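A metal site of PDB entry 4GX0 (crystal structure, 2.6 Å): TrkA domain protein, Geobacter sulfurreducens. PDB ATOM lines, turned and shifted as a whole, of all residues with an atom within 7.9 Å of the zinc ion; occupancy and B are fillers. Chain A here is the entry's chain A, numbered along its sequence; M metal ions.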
ATOM      1  N   HIS A 356      13.894  14.352  23.276  1.00  0.00           N
ATOM      2  CA  HIS A 356      14.072  12.954  23.639  1.00  0.00           C
ATOM      3  C   HIS A 356      15.539  12.581  23.834  1.00  0.00           C
ATOM      4  O   HIS A 356      15.963  11.488  23.495  1.00  0.00           O
ATOM      5  CB  HIS A 356      13.411  12.042  22.610  1.00  0.00           C
ATOM      6  CG  HIS A 356      13.456  10.591  22.970  1.00  0.00           C
ATOM      7  ND1 HIS A 356      13.680   9.585  22.050  1.00  0.00           N
ATOM      8  CD2 HIS A 356      13.316   9.968  24.175  1.00  0.00           C
ATOM      9  CE1 HIS A 356      13.675   8.421  22.657  1.00  0.00           C
ATOM     10  NE2 HIS A 356      13.460   8.619  23.950  1.00  0.00           N
ATOM     11  N   GLY A 357      16.317  13.519  24.370  1.00  0.00           N
ATOM     12  CA  GLY A 357      17.680  13.206  24.783  1.00  0.00           C
ATOM     13  C   GLY A 357      17.630  12.290  25.997  1.00  0.00           C
ATOM     14  O   GLY A 357      16.554  11.830  26.389  1.00  0.00           O
ATOM     15  N   ARG A 358      18.781  12.020  26.604  1.00  0.00           N
ATOM     16  CA  ARG A 358      18.813  11.099  27.732  1.00  0.00           C
ATOM     17  C   ARG A 358      17.903  11.554  28.869  1.00  0.00           C
ATOM     18  O   ARG A 358      17.158  10.759  29.436  1.00  0.00           O
ATOM     19  CB  ARG A 358      20.247  10.905  28.232  1.00  0.00           C
ATOM     20  CG  ARG A 358      21.086  10.008  27.335  1.00  0.00           C
ATOM     21  CD  ARG A 358      22.173   9.301  28.131  1.00  0.00           C
ATOM     22  NE  ARG A 358      22.889   8.329  27.310  1.00  0.00           N
ATOM     23  CZ  ARG A 358      24.009   8.599  26.638  1.00  0.00           C
ATOM     24  NH1 ARG A 358      24.547   9.813  26.712  1.00  0.00           N
ATOM     25  NH2 ARG A 358      24.596   7.652  25.916  1.00  0.00           N
ATOM     26  N   GLY A 360      15.261  13.870  28.819  1.00  0.00           N
ATOM     27  CA  GLY A 360      13.880  13.758  28.376  1.00  0.00           C
ATOM     28  C   GLY A 360      13.415  12.319  28.381  1.00  0.00           C
ATOM     29  O   GLY A 360      12.285  12.013  28.744  1.00  0.00           O
ATOM     30  N   CYS A 361      14.311  11.422  27.964  1.00  0.00           N
ATOM     31  CA  CYS A 361      14.022   9.995  27.945  1.00  0.00           C
ATOM     32  C   CYS A 361      13.790   9.461  29.353  1.00  0.00           C
ATOM     33  O   CYS A 361      12.886   8.661  29.591  1.00  0.00           O
ATOM     34  CB  CYS A 361      15.176   9.234  27.282  1.00  0.00           C
ATOM     35  SG  CYS A 361      14.979   7.439  27.216  1.00  0.00           S
ATOM     36  N   ALA A 362      14.599   9.935  30.302  1.00  0.00           N
ATOM     37  CA  ALA A 362      14.459   9.532  31.697  1.00  0.00           C
ATOM     38  C   ALA A 362      13.138  10.016  32.284  1.00  0.00           C
ATOM     39  O   ALA A 362      12.514   9.307  33.066  1.00  0.00           O
ATOM     40  CB  ALA A 362      15.638  10.049  32.522  1.00  0.00           C
ATOM     41  N   ALA A 363      12.718  11.214  31.911  1.00  0.00           N
ATOM     42  CA  ALA A 363      11.445  11.751  32.388  1.00  0.00           C
ATOM     43  C   ALA A 363      10.296  10.893  31.882  1.00  0.00           C
ATOM     44  O   ALA A 363       9.344  10.616  32.614  1.00  0.00           O
ATOM     45  CB  ALA A 363      11.270  13.198  31.963  1.00  0.00           C
ATOM     46  N   ALA A 364      10.381  10.468  30.615  1.00  0.00           N
ATOM     47  CA  ALA A 364       9.370   9.589  30.048  1.00  0.00           C
ATOM     48  C   ALA A 364       9.331   8.272  30.821  1.00  0.00           C
ATOM     49  O   ALA A 364       8.268   7.829  31.241  1.00  0.00           O
ATOM     50  CB  ALA A 364       9.656   9.332  28.577  1.00  0.00           C
ATOM     51  N   ALA A 365      10.497   7.671  31.002  1.00  0.00           N
ATOM     52  CA  ALA A 365      10.611   6.427  31.755  1.00  0.00           C
ATOM     53  C   ALA A 365       9.967   6.557  33.137  1.00  0.00           C
ATOM     54  O   ALA A 365       9.306   5.635  33.616  1.00  0.00           O
ATOM     55  CB  ALA A 365      12.067   6.004  31.878  1.00  0.00           C
ATOM     56  N   ASP A 368       6.048   6.565  33.063  1.00  0.00           N
ATOM     57  CA  ASP A 368       5.486   5.238  32.846  1.00  0.00           C
ATOM     58  C   ASP A 368       5.124   4.572  34.173  1.00  0.00           C
ATOM     59  O   ASP A 368       4.101   3.906  34.290  1.00  0.00           O
ATOM     60  CB  ASP A 368       6.464   4.345  32.083  1.00  0.00           C
ATOM     61  CG  ASP A 368       6.342   4.509  30.582  1.00  0.00           C
ATOM     62  OD1 ASP A 368       5.210   4.723  30.090  1.00  0.00           O
ATOM     63  OD2 ASP A 368       7.378   4.434  29.887  1.00  0.00           O
ATOM     64  N   PHE A 374       1.766  10.348  28.053  1.00  0.00           N
ATOM     65  CA  PHE A 374       2.644  11.422  27.604  1.00  0.00           C
ATOM     66  C   PHE A 374       3.023  11.252  26.132  1.00  0.00           C
ATOM     67  O   PHE A 374       2.884  10.159  25.578  1.00  0.00           O
ATOM     68  CB  PHE A 374       3.926  11.435  28.448  1.00  0.00           C
ATOM     69  CG  PHE A 374       4.721  10.168  28.336  1.00  0.00           C
ATOM     70  CD1 PHE A 374       5.509   9.921  27.229  1.00  0.00           C
ATOM     71  CD2 PHE A 374       4.680   9.218  29.346  1.00  0.00           C
ATOM     72  CE1 PHE A 374       6.233   8.743  27.122  1.00  0.00           C
ATOM     73  CE2 PHE A 374       5.408   8.045  29.252  1.00  0.00           C
ATOM     74  CZ  PHE A 374       6.181   7.809  28.128  1.00  0.00           C
ATOM     75  N   LEU A 376       6.301  12.069  23.495  1.00  0.00           N
ATOM     76  CA  LEU A 376       7.653  12.535  23.230  1.00  0.00           C
ATOM     77  C   LEU A 376       7.718  13.218  21.875  1.00  0.00           C
ATOM     78  O   LEU A 376       7.156  12.718  20.899  1.00  0.00           O
ATOM     79  CB  LEU A 376       8.638  11.371  23.266  1.00  0.00           C
ATOM     80  CG  LEU A 376       9.063  10.915  24.659  1.00  0.00           C
ATOM     81  CD1 LEU A 376       9.913   9.649  24.602  1.00  0.00           C
ATOM     82  CD2 LEU A 376       9.820  12.042  25.365  1.00  0.00           C
ATOM     83  N   SER A 382      16.360   8.524  18.428  1.00  0.00           N
ATOM     84  CA  SER A 382      17.299   8.336  19.523  1.00  0.00           C
ATOM     85  C   SER A 382      18.321   7.254  19.208  1.00  0.00           C
ATOM     86  O   SER A 382      17.957   6.110  18.949  1.00  0.00           O
ATOM     87  CB  SER A 382      16.552   7.994  20.817  1.00  0.00           C
ATOM     88  OG  SER A 382      17.458   7.881  21.912  1.00  0.00           O
ATOM     89  N   VAL A 384      20.377   5.961  21.243  1.00  0.00           N
ATOM     90  CA  VAL A 384      20.569   5.079  22.396  1.00  0.00           C
ATOM     91  C   VAL A 384      19.260   4.479  22.893  1.00  0.00           C
ATOM     92  O   VAL A 384      19.271   3.533  23.687  1.00  0.00           O
ATOM     93  CB  VAL A 384      21.248   5.818  23.569  1.00  0.00           C
ATOM     94  CG1 VAL A 384      22.548   6.458  23.113  1.00  0.00           C
ATOM     95  CG2 VAL A 384      20.308   6.863  24.157  1.00  0.00           C
ATOM     96  N   CYS A 385      18.138   5.013  22.425  1.00  0.00           N
ATOM     97  CA  CYS A 385      16.837   4.544  22.885  1.00  0.00           C
ATOM     98  C   CYS A 385      15.967   3.986  21.767  1.00  0.00           C
ATOM     99  O   CYS A 385      15.950   4.516  20.656  1.00  0.00           O
ATOM    100  CB  CYS A 385      16.074   5.667  23.604  1.00  0.00           C
ATOM    101  SG  CYS A 385      14.379   5.237  24.040  1.00  0.00           S
ATOM    102  N   ASN A 386      15.243   2.909  22.085  1.00  0.00           N
ATOM    103  CA  ASN A 386      14.321   2.286  21.138  1.00  0.00           C
ATOM    104  C   ASN A 386      13.096   1.707  21.834  1.00  0.00           C
ATOM    105  O   ASN A 386      12.351   0.926  21.250  1.00  0.00           O
ATOM    106  CB  ASN A 386      15.031   1.192  20.333  1.00  0.00           C
ATOM    107  CG  ASN A 386      16.169   1.747  19.481  1.00  0.00           C
ATOM    108  OD1 ASN A 386      17.341   1.449  19.727  1.00  0.00           O
ATOM    109  ND2 ASN A 386      15.831   2.558  18.482  1.00  0.00           N
ATOM    110  N   ASP A 387      12.886   2.108  23.091  1.00  0.00           N
ATOM    111  CA  ASP A 387      11.774   1.590  23.879  1.00  0.00           C
ATOM    112  C   ASP A 387      10.638   2.605  23.993  1.00  0.00           C
ATOM    113  O   ASP A 387       9.605   2.320  24.615  1.00  0.00           O
ATOM    114  CB  ASP A 387      12.263   1.203  25.279  1.00  0.00           C
ATOM    115  CG  ASP A 387      13.412   0.229  25.248  1.00  0.00           C
ATOM    116  OD1 ASP A 387      14.407   0.452  25.976  1.00  0.00           O
ATOM    117  OD2 ASP A 387      13.340  -0.762  24.486  1.00  0.00           O
ATOM    118  N   HIS A 388      10.828   3.771  23.388  1.00  0.00           N
ATOM    119  CA  HIS A 388       9.820   4.825  23.415  1.00  0.00           C
ATOM    120  C   HIS A 388       9.364   5.208  22.007  1.00  0.00           C
ATOM    121  O   HIS A 388      10.157   5.204  21.071  1.00  0.00           O
ATOM    122  CB  HIS A 388      10.341   6.070  24.144  1.00  0.00           C
ATOM    123  CG  HIS A 388      10.245   5.982  25.643  1.00  0.00           C
ATOM    124  ND1 HIS A 388      11.276   6.341  26.476  1.00  0.00           N
ATOM    125  CD2 HIS A 388       9.220   5.601  26.449  1.00  0.00           C
ATOM    126  CE1 HIS A 388      10.910   6.169  27.729  1.00  0.00           C
ATOM    127  NE2 HIS A 388       9.665   5.724  27.747  1.00  0.00           N
ATOM    128  N   VAL A 389       8.082   5.521  21.867  1.00  0.00           N
ATOM    129  CA  VAL A 389       7.566   6.050  20.612  1.00  0.00           C
ATOM    130  C   VAL A 389       7.759   7.559  20.581  1.00  0.00           C
ATOM    131  O   VAL A 389       7.382   8.248  21.526  1.00  0.00           O
ATOM    132  CB  VAL A 389       6.077   5.736  20.433  1.00  0.00           C
ATOM    133  CG1 VAL A 389       5.552   6.348  19.143  1.00  0.00           C
ATOM    134  CG2 VAL A 389       5.833   4.236  20.442  1.00  0.00           C
ATOM    135  N   VAL A 390       8.334   8.059  19.490  1.00  0.00           N
ATOM    136  CA  VAL A 390       8.624   9.490  19.379  1.00  0.00           C
ATOM    137  C   VAL A 390       7.945  10.117  18.166  1.00  0.00           C
ATOM    138  O   VAL A 390       8.125   9.658  17.047  1.00  0.00           O
ATOM    139  CB  VAL A 390      10.139   9.752  19.285  1.00  0.00           C
ATOM    140  CG1 VAL A 390      10.408  11.219  19.036  1.00  0.00           C
ATOM    141  CG2 VAL A 390      10.837   9.274  20.554  1.00  0.00           C
HETATM  142 ZN    ZN M   1      13.233   6.915  25.437  1.00  0.00          ZN
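N of Asp 387 sits close to SG of Cys 385, at 3.6 Å.
A ring nitrogen (NE2) of His 388 sits at hydrogen-bond distance from the side-chain carboxylate (OD2) of Asp 368 (3.4 Å).
The backbone NH of Cys 385 lies within hydrogen-bond range of the side-chain hydroxyl of Ser 382 (3.0 Å).
Within 4 Å of the zinc ion: His 356, Cys 361, Cys 385 and His 388.
The zinc ion is bound by a ring nitrogen (NE2) of His 356 (2.3 Å), a ring nitrogen (ND1) of His 388 (2.3 Å), the side-chain sulfur (SG) of Cys 385 (2.5 Å) and the side-chain sulfur (SG) of Cys 361 (2.5 Å).
The zinc ion has four donor atoms within binding distance.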
